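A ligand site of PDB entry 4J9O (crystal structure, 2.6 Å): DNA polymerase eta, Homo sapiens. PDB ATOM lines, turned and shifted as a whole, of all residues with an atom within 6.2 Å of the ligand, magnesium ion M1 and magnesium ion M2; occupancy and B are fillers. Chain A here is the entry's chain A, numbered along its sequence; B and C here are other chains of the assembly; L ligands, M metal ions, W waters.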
ATOM      1  N   ASP A  16     -31.769  23.794  35.261  1.00  0.00           N
ATOM      2  CA  ASP A  16     -31.293  22.799  34.300  1.00  0.00           C
ATOM      3  C   ASP A  16     -30.960  21.479  34.986  1.00  0.00           C
ATOM      4  O   ASP A  16     -30.102  21.411  35.869  1.00  0.00           O
ATOM      5  CB  ASP A  16     -30.057  23.298  33.547  1.00  0.00           C
ATOM      6  CG  ASP A  16     -29.541  22.289  32.523  1.00  0.00           C
ATOM      7  OD1 ASP A  16     -28.821  21.336  32.925  1.00  0.00           O
ATOM      8  OD2 ASP A  16     -29.853  22.438  31.328  1.00  0.00           O
ATOM      9  N   MET A  17     -31.646  20.430  34.543  1.00  0.00           N
ATOM     10  CA  MET A  17     -31.455  19.106  35.115  1.00  0.00           C
ATOM     11  C   MET A  17     -30.040  18.597  34.893  1.00  0.00           C
ATOM     12  O   MET A  17     -29.455  18.735  33.821  1.00  0.00           O
ATOM     13  CB  MET A  17     -32.495  18.150  34.556  1.00  0.00           C
ATOM     14  CG  MET A  17     -33.894  18.774  34.437  1.00  0.00           C
ATOM     15  SD  MET A  17     -34.664  19.122  36.036  1.00  0.00           S
ATOM     16  CE  MET A  17     -34.251  17.599  36.893  1.00  0.00           C
ATOM     17  N   ASP A  18     -29.499  18.024  35.951  1.00  0.00           N
ATOM     18  CA  ASP A  18     -28.190  17.392  35.922  1.00  0.00           C
ATOM     19  C   ASP A  18     -28.263  16.074  35.160  1.00  0.00           C
ATOM     20  O   ASP A  18     -29.068  15.196  35.485  1.00  0.00           O
ATOM     21  CB  ASP A  18     -27.717  17.188  37.357  1.00  0.00           C
ATOM     22  CG  ASP A  18     -27.559  18.506  38.089  1.00  0.00           C
ATOM     23  OD1 ASP A  18     -27.395  19.525  37.387  1.00  0.00           O
ATOM     24  OD2 ASP A  18     -27.597  18.525  39.344  1.00  0.00           O
ATOM     25  N   CYS A  19     -27.417  15.965  34.139  1.00  0.00           N
ATOM     26  CA  CYS A  19     -27.333  14.812  33.231  1.00  0.00           C
ATOM     27  C   CYS A  19     -28.653  14.089  32.996  1.00  0.00           C
ATOM     28  O   CYS A  19     -28.736  12.866  33.124  1.00  0.00           O
ATOM     29  CB  CYS A  19     -26.219  13.856  33.678  1.00  0.00           C
ATOM     30  SG  CYS A  19     -26.199  13.425  35.436  1.00  0.00           S
ATOM     31  N   PHE A  20     -29.650  14.871  32.582  1.00  0.00           N
ATOM     32  CA  PHE A  20     -31.054  14.472  32.564  1.00  0.00           C
ATOM     33  C   PHE A  20     -31.386  13.053  32.086  1.00  0.00           C
ATOM     34  O   PHE A  20     -32.012  12.281  32.817  1.00  0.00           O
ATOM     35  CB  PHE A  20     -31.902  15.508  31.811  1.00  0.00           C
ATOM     36  CG  PHE A  20     -33.372  15.307  31.985  1.00  0.00           C
ATOM     37  CD1 PHE A  20     -33.916  15.122  33.248  1.00  0.00           C
ATOM     38  CD2 PHE A  20     -34.220  15.306  30.893  1.00  0.00           C
ATOM     39  CE1 PHE A  20     -35.277  14.935  33.415  1.00  0.00           C
ATOM     40  CE2 PHE A  20     -35.593  15.115  31.051  1.00  0.00           C
ATOM     41  CZ  PHE A  20     -36.114  14.938  32.316  1.00  0.00           C
ATOM     42  N   PHE A  21     -30.975  12.706  30.865  1.00  0.00           N
ATOM     43  CA  PHE A  21     -31.314  11.396  30.321  1.00  0.00           C
ATOM     44  C   PHE A  21     -30.747  10.269  31.195  1.00  0.00           C
ATOM     45  O   PHE A  21     -31.356   9.210  31.316  1.00  0.00           O
ATOM     46  CB  PHE A  21     -30.826  11.249  28.873  1.00  0.00           C
ATOM     47  CG  PHE A  21     -31.656  12.017  27.866  1.00  0.00           C
ATOM     48  CD1 PHE A  21     -32.435  13.102  28.240  1.00  0.00           C
ATOM     49  CD2 PHE A  21     -31.629  11.654  26.522  1.00  0.00           C
ATOM     50  CE1 PHE A  21     -33.190  13.816  27.291  1.00  0.00           C
ATOM     51  CE2 PHE A  21     -32.369  12.349  25.572  1.00  0.00           C
ATOM     52  CZ  PHE A  21     -33.148  13.433  25.961  1.00  0.00           C
ATOM     53  N   VAL A  22     -29.588  10.519  31.800  1.00  0.00           N
ATOM     54  CA  VAL A  22     -28.956   9.554  32.722  1.00  0.00           C
ATOM     55  C   VAL A  22     -29.761   9.373  34.034  1.00  0.00           C
ATOM     56  O   VAL A  22     -30.010   8.236  34.456  1.00  0.00           O
ATOM     57  CB  VAL A  22     -27.506   9.977  33.041  1.00  0.00           C
ATOM     58  CG1 VAL A  22     -26.919   9.096  34.114  1.00  0.00           C
ATOM     59  CG2 VAL A  22     -26.635   9.959  31.779  1.00  0.00           C
ATOM     60  N   GLN A  41     -27.356   5.616  21.908  1.00  0.00           N
ATOM     61  CA  GLN A  41     -28.361   5.231  20.936  1.00  0.00           C
ATOM     62  C   GLN A  41     -27.668   4.596  19.729  1.00  0.00           C
ATOM     63  O   GLN A  41     -26.559   5.000  19.376  1.00  0.00           O
ATOM     64  CB  GLN A  41     -29.203   6.448  20.505  1.00  0.00           C
ATOM     65  CG  GLN A  41     -28.420   7.552  19.779  1.00  0.00           C
ATOM     66  CD  GLN A  41     -29.292   8.744  19.416  1.00  0.00           C
ATOM     67  OE1 GLN A  41     -30.333   8.986  20.043  1.00  0.00           O
ATOM     68  NE2 GLN A  41     -28.878   9.499  18.410  1.00  0.00           N
ATOM     69  N   ILE A  51     -25.231  10.449  24.141  1.00  0.00           N
ATOM     70  CA  ILE A  51     -25.944  11.720  24.224  1.00  0.00           C
ATOM     71  C   ILE A  51     -26.083  12.249  25.649  1.00  0.00           C
ATOM     72  O   ILE A  51     -26.542  13.372  25.859  1.00  0.00           O
ATOM     73  CB  ILE A  51     -27.333  11.642  23.572  1.00  0.00           C
ATOM     74  CG1 ILE A  51     -28.134  10.493  24.180  1.00  0.00           C
ATOM     75  CG2 ILE A  51     -27.221  11.479  22.066  1.00  0.00           C
ATOM     76  CD1 ILE A  51     -29.494  10.301  23.552  1.00  0.00           C
ATOM     77  N   ALA A  52     -25.689  11.443  26.629  1.00  0.00           N
ATOM     78  CA  ALA A  52     -25.763  11.868  28.023  1.00  0.00           C
ATOM     79  C   ALA A  52     -24.754  11.124  28.907  1.00  0.00           C
ATOM     80  O   ALA A  52     -24.665   9.894  28.861  1.00  0.00           O
ATOM     81  CB  ALA A  52     -27.186  11.702  28.556  1.00  0.00           C
ATOM     82  N   VAL A  53     -24.012  11.874  29.714  1.00  0.00           N
ATOM     83  CA  VAL A  53     -22.947  11.318  30.534  1.00  0.00           C
ATOM     84  C   VAL A  53     -23.150  11.669  32.016  1.00  0.00           C
ATOM     85  O   VAL A  53     -23.429  12.822  32.352  1.00  0.00           O
ATOM     86  CB  VAL A  53     -21.581  11.877  30.075  1.00  0.00           C
ATOM     87  CG1 VAL A  53     -20.427  11.131  30.720  1.00  0.00           C
ATOM     88  CG2 VAL A  53     -21.476  11.836  28.561  1.00  0.00           C
ATOM     89  N   TYR A  55     -21.873  12.386  35.895  1.00  0.00           N
ATOM     90  CA  TYR A  55     -20.702  13.098  36.370  1.00  0.00           C
ATOM     91  C   TYR A  55     -19.539  12.156  36.727  1.00  0.00           C
ATOM     92  O   TYR A  55     -18.380  12.453  36.428  1.00  0.00           O
ATOM     93  CB  TYR A  55     -21.071  14.057  37.513  1.00  0.00           C
ATOM     94  CG  TYR A  55     -21.721  15.309  36.974  1.00  0.00           C
ATOM     95  CD1 TYR A  55     -23.045  15.313  36.571  1.00  0.00           C
ATOM     96  CD2 TYR A  55     -20.982  16.494  36.839  1.00  0.00           C
ATOM     97  CE1 TYR A  55     -23.633  16.458  36.059  1.00  0.00           C
ATOM     98  CE2 TYR A  55     -21.560  17.636  36.328  1.00  0.00           C
ATOM     99  CZ  TYR A  55     -22.892  17.618  35.944  1.00  0.00           C
ATOM    100  OH  TYR A  55     -23.470  18.760  35.433  1.00  0.00           O
ATOM    101  N   ARG A  58     -17.781  11.485  33.744  1.00  0.00           N
ATOM    102  CA  ARG A  58     -17.041  12.657  33.261  1.00  0.00           C
ATOM    103  C   ARG A  58     -15.653  12.767  33.886  1.00  0.00           C
ATOM    104  O   ARG A  58     -14.737  13.331  33.274  1.00  0.00           O
ATOM    105  CB  ARG A  58     -17.851  13.943  33.509  1.00  0.00           C
ATOM    106  CG  ARG A  58     -19.164  13.969  32.753  1.00  0.00           C
ATOM    107  CD  ARG A  58     -19.915  15.272  32.949  1.00  0.00           C
ATOM    108  NE  ARG A  58     -21.331  15.143  32.598  1.00  0.00           N
ATOM    109  CZ  ARG A  58     -22.154  16.170  32.406  1.00  0.00           C
ATOM    110  NH1 ARG A  58     -21.728  17.425  32.526  1.00  0.00           N
ATOM    111  NH2 ARG A  58     -23.426  15.932  32.092  1.00  0.00           N
ATOM    112  N   ARG A  64     -20.389  13.740  25.577  1.00  0.00           N
ATOM    113  CA  ARG A  64     -21.437  13.530  24.597  1.00  0.00           C
ATOM    114  C   ARG A  64     -20.891  13.665  23.189  1.00  0.00           C
ATOM    115  O   ARG A  64     -19.917  14.379  22.957  1.00  0.00           O
ATOM    116  CB  ARG A  64     -22.592  14.511  24.802  1.00  0.00           C
ATOM    117  CG  ARG A  64     -22.579  15.687  23.837  1.00  0.00           C
ATOM    118  CD  ARG A  64     -23.872  15.782  23.057  1.00  0.00           C
ATOM    119  NE  ARG A  64     -23.729  16.457  21.775  1.00  0.00           N
ATOM    120  CZ  ARG A  64     -23.162  17.649  21.602  1.00  0.00           C
ATOM    121  NH1 ARG A  64     -23.084  18.182  20.401  1.00  0.00           N
ATOM    122  NH2 ARG A  64     -22.676  18.308  22.645  1.00  0.00           N
ATOM    123  N   SER A 116     -35.610  24.164  26.809  1.00  0.00           N
ATOM    124  CA  SER A 116     -35.203  22.874  26.232  1.00  0.00           C
ATOM    125  C   SER A 116     -35.966  21.766  26.944  1.00  0.00           C
ATOM    126  O   SER A 116     -36.780  22.037  27.819  1.00  0.00           O
ATOM    127  CB  SER A 116     -33.704  22.646  26.392  1.00  0.00           C
ATOM    128  OG  SER A 116     -33.435  21.906  27.581  1.00  0.00           O
ATOM    129  N   ILE A 117     -35.682  20.518  26.582  1.00  0.00           N
ATOM    130  CA  ILE A 117     -36.335  19.383  27.228  1.00  0.00           C
ATOM    131  C   ILE A 117     -35.961  19.241  28.710  1.00  0.00           C
ATOM    132  O   ILE A 117     -36.754  18.732  29.502  1.00  0.00           O
ATOM    133  CB  ILE A 117     -36.032  18.069  26.480  1.00  0.00           C
ATOM    134  CG1 ILE A 117     -36.799  16.901  27.111  1.00  0.00           C
ATOM    135  CG2 ILE A 117     -34.534  17.810  26.454  1.00  0.00           C
ATOM    136  CD1 ILE A 117     -36.669  15.599  26.347  1.00  0.00           C
ATOM    137  N   ASP A 118     -34.778  19.720  29.088  1.00  0.00           N
ATOM    138  CA  ASP A 118     -34.335  19.623  30.478  1.00  0.00           C
ATOM    139  C   ASP A 118     -34.138  20.969  31.192  1.00  0.00           C
ATOM    140  O   ASP A 118     -33.545  21.021  32.265  1.00  0.00           O
ATOM    141  CB  ASP A 118     -33.071  18.781  30.584  1.00  0.00           C
ATOM    142  CG  ASP A 118     -31.811  19.589  30.374  1.00  0.00           C
ATOM    143  OD1 ASP A 118     -31.732  20.335  29.376  1.00  0.00           O
ATOM    144  OD2 ASP A 118     -30.903  19.472  31.223  1.00  0.00           O
ATOM    145  N   GLU A 119     -34.647  22.051  30.610  1.00  0.00           N
ATOM    146  CA  GLU A 119     -34.470  23.355  31.258  1.00  0.00           C
ATOM    147  C   GLU A 119     -35.544  24.353  30.901  1.00  0.00           C
ATOM    148  O   GLU A 119     -36.075  24.367  29.786  1.00  0.00           O
ATOM    149  CB  GLU A 119     -33.086  23.928  30.957  1.00  0.00           C
ATOM    150  CG  GLU A 119     -32.951  24.523  29.585  1.00  0.00           C
ATOM    151  CD  GLU A 119     -31.521  24.542  29.123  1.00  0.00           C
ATOM    152  OE1 GLU A 119     -30.954  23.448  28.999  1.00  0.00           O
ATOM    153  OE2 GLU A 119     -30.960  25.637  28.902  1.00  0.00           O
ATOM    154  N   SER A 216     -29.459  21.874  38.762  1.00  0.00           N
ATOM    155  CA  SER A 216     -28.756  23.111  39.095  1.00  0.00           C
ATOM    156  C   SER A 216     -29.546  24.318  38.610  1.00  0.00           C
ATOM    157  O   SER A 216     -30.389  24.220  37.719  1.00  0.00           O
ATOM    158  CB  SER A 216     -27.359  23.099  38.467  1.00  0.00           C
ATOM    159  OG  SER A 216     -26.627  21.972  38.896  1.00  0.00           O
ATOM    160  N   LYS A 234     -21.998  23.104  39.197  1.00  0.00           N
ATOM    161  CA  LYS A 234     -22.728  21.881  38.884  1.00  0.00           C
ATOM    162  C   LYS A 234     -21.995  20.665  39.415  1.00  0.00           C
ATOM    163  O   LYS A 234     -20.760  20.664  39.501  1.00  0.00           O
ATOM    164  CB  LYS A 234     -22.903  21.734  37.369  1.00  0.00           C
ATOM    165  CG  LYS A 234     -24.178  22.361  36.811  1.00  0.00           C
ATOM    166  CD  LYS A 234     -24.493  21.812  35.401  1.00  0.00           C
ATOM    167  CE  LYS A 234     -25.827  22.344  34.855  1.00  0.00           C
ATOM    168  NZ  LYS A 234     -26.985  21.418  35.079  1.00  0.00           N
ATOM    169  N   PRO A 235     -22.745  19.616  39.755  1.00  0.00           N
ATOM    170  CA  PRO A 235     -24.214  19.543  39.779  1.00  0.00           C
ATOM    171  C   PRO A 235     -24.851  19.812  41.140  1.00  0.00           C
ATOM    172  O   PRO A 235     -24.157  20.130  42.112  1.00  0.00           O
ATOM    173  CB  PRO A 235     -24.478  18.084  39.388  1.00  0.00           C
ATOM    174  CG  PRO A 235     -23.306  17.347  39.928  1.00  0.00           C
ATOM    175  CD  PRO A 235     -22.131  18.271  39.768  1.00  0.00           C
ATOM    176  P    DG B   9     -26.767  25.312  24.830  1.00  0.00           P
ATOM    177  OP1  DG B   9     -26.135  25.983  25.953  1.00  0.00           O
ATOM    178  OP2  DG B   9     -25.957  24.481  23.953  1.00  0.00           O
ATOM    179  O5'  DG B   9     -27.912  24.473  25.549  1.00  0.00           O
ATOM    180  C5'  DG B   9     -29.277  24.506  25.102  1.00  0.00           C
ATOM    181  C4'  DG B   9     -29.838  23.110  25.010  1.00  0.00           C
ATOM    182  O4'  DG B   9     -29.751  22.628  23.648  1.00  0.00           O
ATOM    183  C3'  DG B   9     -29.109  22.072  25.855  1.00  0.00           C
ATOM    184  O3'  DG B   9     -29.996  21.512  26.802  1.00  0.00           O
ATOM    185  C2'  DG B   9     -28.612  21.037  24.857  1.00  0.00           C
ATOM    186  C1'  DG B   9     -29.533  21.245  23.694  1.00  0.00           C
ATOM    187  N9   DG B   9     -29.061  20.805  22.392  1.00  0.00           N
ATOM    188  C8   DG B   9     -27.955  21.220  21.684  1.00  0.00           C
ATOM    189  N7   DG B   9     -27.830  20.609  20.531  1.00  0.00           N
ATOM    190  C5   DG B   9     -28.909  19.738  20.493  1.00  0.00           C
ATOM    191  C6   DG B   9     -29.306  18.816  19.485  1.00  0.00           C
ATOM    192  O6   DG B   9     -28.758  18.568  18.404  1.00  0.00           O
ATOM    193  N1   DG B   9     -30.455  18.128  19.849  1.00  0.00           N
ATOM    194  C2   DG B   9     -31.146  18.323  21.018  1.00  0.00           C
ATOM    195  N2   DG B   9     -32.253  17.570  21.190  1.00  0.00           N
ATOM    196  N3   DG B   9     -30.796  19.182  21.957  1.00  0.00           N
ATOM    197  C4   DG B   9     -29.674  19.853  21.625  1.00  0.00           C
ATOM    198  P    DT C   4     -24.306  12.106  13.105  1.00  0.00           P
ATOM    199  OP1  DT C   4     -23.441  11.315  12.198  1.00  0.00           O
ATOM    200  OP2  DT C   4     -24.581  13.544  12.825  1.00  0.00           O
ATOM    201  O5'  DT C   4     -25.715  11.345  13.252  1.00  0.00           O
ATOM    202  C5'  DT C   4     -25.803  10.131  14.012  1.00  0.00           C
ATOM    203  C4'  DT C   4     -27.067  10.097  14.866  1.00  0.00           C
ATOM    204  O4'  DT C   4     -26.899  11.002  16.002  1.00  0.00           O
ATOM    205  C3'  DT C   4     -28.338  10.534  14.162  1.00  0.00           C
ATOM    206  O3'  DT C   4     -29.403   9.745  14.583  1.00  0.00           O
ATOM    207  C2'  DT C   4     -28.500  12.001  14.593  1.00  0.00           C
ATOM    208  C1'  DT C   4     -27.966  11.935  16.018  1.00  0.00           C
ATOM    209  N1   DT C   4     -27.470  13.212  16.597  1.00  0.00           N
ATOM    210  C2   DT C   4     -28.065  13.638  17.763  1.00  0.00           C
ATOM    211  O2   DT C   4     -28.959  13.033  18.324  1.00  0.00           O
ATOM    212  N3   DT C   4     -27.565  14.810  18.259  1.00  0.00           N
ATOM    213  C4   DT C   4     -26.553  15.578  17.720  1.00  0.00           C
ATOM    214  O4   DT C   4     -26.184  16.622  18.258  1.00  0.00           O
ATOM    215  C5   DT C   4     -25.976  15.080  16.500  1.00  0.00           C
ATOM    216  C7   DT C   4     -24.872  15.824  15.831  1.00  0.00           C
ATOM    217  C6   DT C   4     -26.451  13.924  15.999  1.00  0.00           C
ATOM    218  P    DT C   5     -30.897   9.960  13.955  1.00  0.00           P
ATOM    219  OP1  DT C   5     -31.607   8.678  13.980  1.00  0.00           O
ATOM    220  OP2  DT C   5     -30.708  10.687  12.685  1.00  0.00           O
ATOM    221  O5'  DT C   5     -31.598  10.977  14.983  1.00  0.00           O
ATOM    222  C5'  DT C   5     -32.086  10.512  16.235  1.00  0.00           C
ATOM    223  C4'  DT C   5     -32.748  11.662  16.995  1.00  0.00           C
ATOM    224  O4'  DT C   5     -31.770  12.718  17.229  1.00  0.00           O
ATOM    225  C3'  DT C   5     -33.924  12.318  16.259  1.00  0.00           C
ATOM    226  O3'  DT C   5     -34.923  12.607  17.210  1.00  0.00           O
ATOM    227  C2'  DT C   5     -33.313  13.617  15.747  1.00  0.00           C
ATOM    228  C1'  DT C   5     -32.341  13.949  16.878  1.00  0.00           C
ATOM    229  N1   DT C   5     -31.268  14.875  16.458  1.00  0.00           N
ATOM    230  C2   DT C   5     -30.808  15.787  17.370  1.00  0.00           C
ATOM    231  O2   DT C   5     -31.230  15.863  18.506  1.00  0.00           O
ATOM    232  N3   DT C   5     -29.806  16.603  16.912  1.00  0.00           N
ATOM    233  C4   DT C   5     -29.244  16.598  15.660  1.00  0.00           C
ATOM    234  O4   DT C   5     -28.349  17.390  15.364  1.00  0.00           O
ATOM    235  C5   DT C   5     -29.775  15.619  14.740  1.00  0.00           C
ATOM    236  C7   DT C   5     -29.227  15.540  13.342  1.00  0.00           C
ATOM    237  C6   DT C   5     -30.754  14.805  15.179  1.00  0.00           C
HETATM  238  N1  LIG L   1     -27.948  15.638  20.806  1.00  0.00           N
HETATM  239  C1  LIG L   1     -28.877  14.827  21.311  1.00  0.00           C
HETATM  240  N2  LIG L   1     -29.388  14.826  22.544  1.00  0.00           N
HETATM  241  C2  LIG L   1     -28.855  15.793  23.315  1.00  0.00           C
HETATM  242  C3  LIG L   1     -27.890  16.705  22.916  1.00  0.00           C
HETATM  243  C4  LIG L   1     -27.426  16.600  21.582  1.00  0.00           C
HETATM  244  N3  LIG L   1     -26.487  17.409  21.077  1.00  0.00           N
HETATM  245  N4  LIG L   1     -27.567  17.557  23.959  1.00  0.00           N
HETATM  246  C5  LIG L   1     -28.335  17.167  24.950  1.00  0.00           C
HETATM  247  N5  LIG L   1     -29.135  16.104  24.634  1.00  0.00           N
HETATM  248  P1  LIG L   1     -27.892  19.196  28.595  1.00  0.00           P
HETATM  249  P2  LIG L   1     -27.248  17.174  30.695  1.00  0.00           P
HETATM  250  P3  LIG L   1     -25.671  18.624  32.453  1.00  0.00           P
HETATM  251  C6  LIG L   1     -30.098  15.452  25.529  1.00  0.00           C
HETATM  252  O1  LIG L   1     -28.325  20.004  29.748  1.00  0.00           O
HETATM  253  O2  LIG L   1     -28.527  17.495  31.369  1.00  0.00           O
HETATM  254  O3  LIG L   1     -26.600  19.744  32.189  1.00  0.00           O
HETATM  255  C7  LIG L   1     -29.504  14.435  26.517  1.00  0.00           C
HETATM  256  O4  LIG L   1     -27.259  19.934  27.480  1.00  0.00           O
HETATM  257  O5  LIG L   1     -27.152  15.764  30.257  1.00  0.00           O
HETATM  258  O6  LIG L   1     -25.705  18.618  33.940  1.00  0.00           O
HETATM  259  C8  LIG L   1     -29.242  15.252  27.774  1.00  0.00           C
HETATM  260  O7  LIG L   1     -29.221  14.563  29.023  1.00  0.00           O
HETATM  261  N6  LIG L   1     -26.933  18.030  29.291  1.00  0.00           N
HETATM  262  O8  LIG L   1     -26.366  17.479  31.827  1.00  0.00           O
HETATM  263  O9  LIG L   1     -24.296  18.808  31.954  1.00  0.00           O
HETATM  264  C9  LIG L   1     -30.290  16.348  27.715  1.00  0.00           C
HETATM  265  O10 LIG L   1     -30.711  16.453  26.327  1.00  0.00           O
HETATM  266  C10 LIG L   1     -30.076  17.591  28.553  1.00  0.00           C
HETATM  267  O11 LIG L   1     -29.309  18.670  28.038  1.00  0.00           O
HETATM  268 MG    MG M   1     -28.958  19.463  31.931  1.00  0.00          MG
HETATM  269 MG    MG M   2     -29.687  21.561  29.397  1.00  0.00          MG
HETATM  270  O   HOH W   1     -23.640  18.961  29.326  1.00  0.00           O
HETATM  271  O   HOH W   2     -24.779  14.730  29.453  1.00  0.00           O
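The guanidinium group (NE) of Arg 64 lies close to a nitrogen (N3) of the ligand (3.0 Å). Asp 18 touches the ligand (CA to O6, 3.4 Å). O of Ile 51 touches C7 of the ligand, 3.2 Å away. Ala 52 touches the ligand (CB to O7, 3.5 Å). DT 5 of chain C touches the ligand (O2 to C1, 3.8 Å). Hydrophobic or aromatic side chains within 4 Å of the ligand: Phe 20, Phe 21, Ile 51, Ala 52 and Tyr 55. Within 4 Å of the ligand: Asp 16, Met 17, Asp 18, Cys 19, Phe 20, Phe 21, Ile 51, Ala 52, Tyr 55, Arg 58, Arg 64, Asp 118, Lys 234, DG 9 of chain B, DT 4 of chain C and DT 5 of chain C.
The side-chain carboxylate (OD2) of Asp 118 is bound to magnesium ion M1 (2.1 Å). O of Met 17 is bound to magnesium ion M1 (2.1 Å). O2 of the ligand is bound to magnesium ion M1 (2.1 Å). OD1 of Asp 16 binds magnesium ion M1, 2.1 Å away. O1 of the ligand binds magnesium ion M1 (2.3 Å). O3 of the ligand binds magnesium ion M1, at 2.4 Å. Magnesium ion M1 has six donor atoms within binding distance.
Within 4 Å of magnesium ion M1: Asp 16, Met 17 and Asp 118. The nearest printed residue that does not touch magnesium ion M1 is Lys 234 (4.2 Å).
Four residues have an atom within 4 Å of magnesium ion M2: Asp 16, Asp 118, Glu 119 and DG 9 of chain B.
O1 of the ligand binds magnesium ion M2 (2.1 Å). Magnesium ion M2 is bound by the side-chain carboxylate (OD2) of Asp 16, 2.1 Å away. Magnesium ion M2 is bound by OE1 of Glu 119. Magnesium ion M2 is bound by OD1 of Asp 118. Slightly farther from magnesium ion M2 lies O3' of DG 9 of chain B (2.6 Å).
Water W2 lies within hydrogen-bond range of an oxygen (O5) of the ligand (2.7 Å), the backbone NH (N) of Val 53 (3.0 Å) and the guanidinium group (NH2) of Arg 58 (3.2 Å).
The side-chain amino group (NZ) of Lys 234 lies within salt-bridge range of the side-chain carboxylate (OD1) of Asp 18 (3.0 Å). OG of Ser 116 sits at hydrogen-bond distance from N of Glu 119 (3.3 Å). The backbone carbonyl oxygen (O) of Asp 16 lies within hydrogen-bond range of the side-chain amino group (NZ) of Lys 234, 3.2 Å away. The guanidinium group of Arg 58 lies within hydrogen-bond range of the backbone carbonyl oxygen of Val 53 (3.1 Å). O6 of DG 9 of chain B lies close to N3 of DT 5 of chain C (2.7 Å). The side-chain carboxylate of Asp 18 is in hydrogen-bond range of the side-chain hydroxyl of Ser 216 (3.0 Å). O4' of DT 4 of chain C sits at hydrogen-bond distance from NE2 of Gln 41 (3.5 Å). O of Ser 216 sits at hydrogen-bond distance from N of Asp 16 (2.9 Å).
An oxygen (O2) of the ligand sits close to the backbone NH (N) of Phe 20, 3.1 Å away. An oxygen (O7) of the ligand is in hydrogen-bond range of the backbone NH of Phe 21 (3.1 Å). NZ of Lys 234 is in salt-bridge range of O6 of the ligand (3.3 Å). OH of Tyr 55 is in hydrogen-bond range of O6 of the ligand. The backbone NH of Cys 19 is in hydrogen-bond range of an oxygen (O8) of the ligand (3.0 Å). An oxygen (O9) of the ligand is in salt-bridge range of the guanidinium group (NH1) of Arg 58 (3.0 Å). O4 of DT 4 of chain C lies within hydrogen-bond range of N3 of the ligand (2.9 Å).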
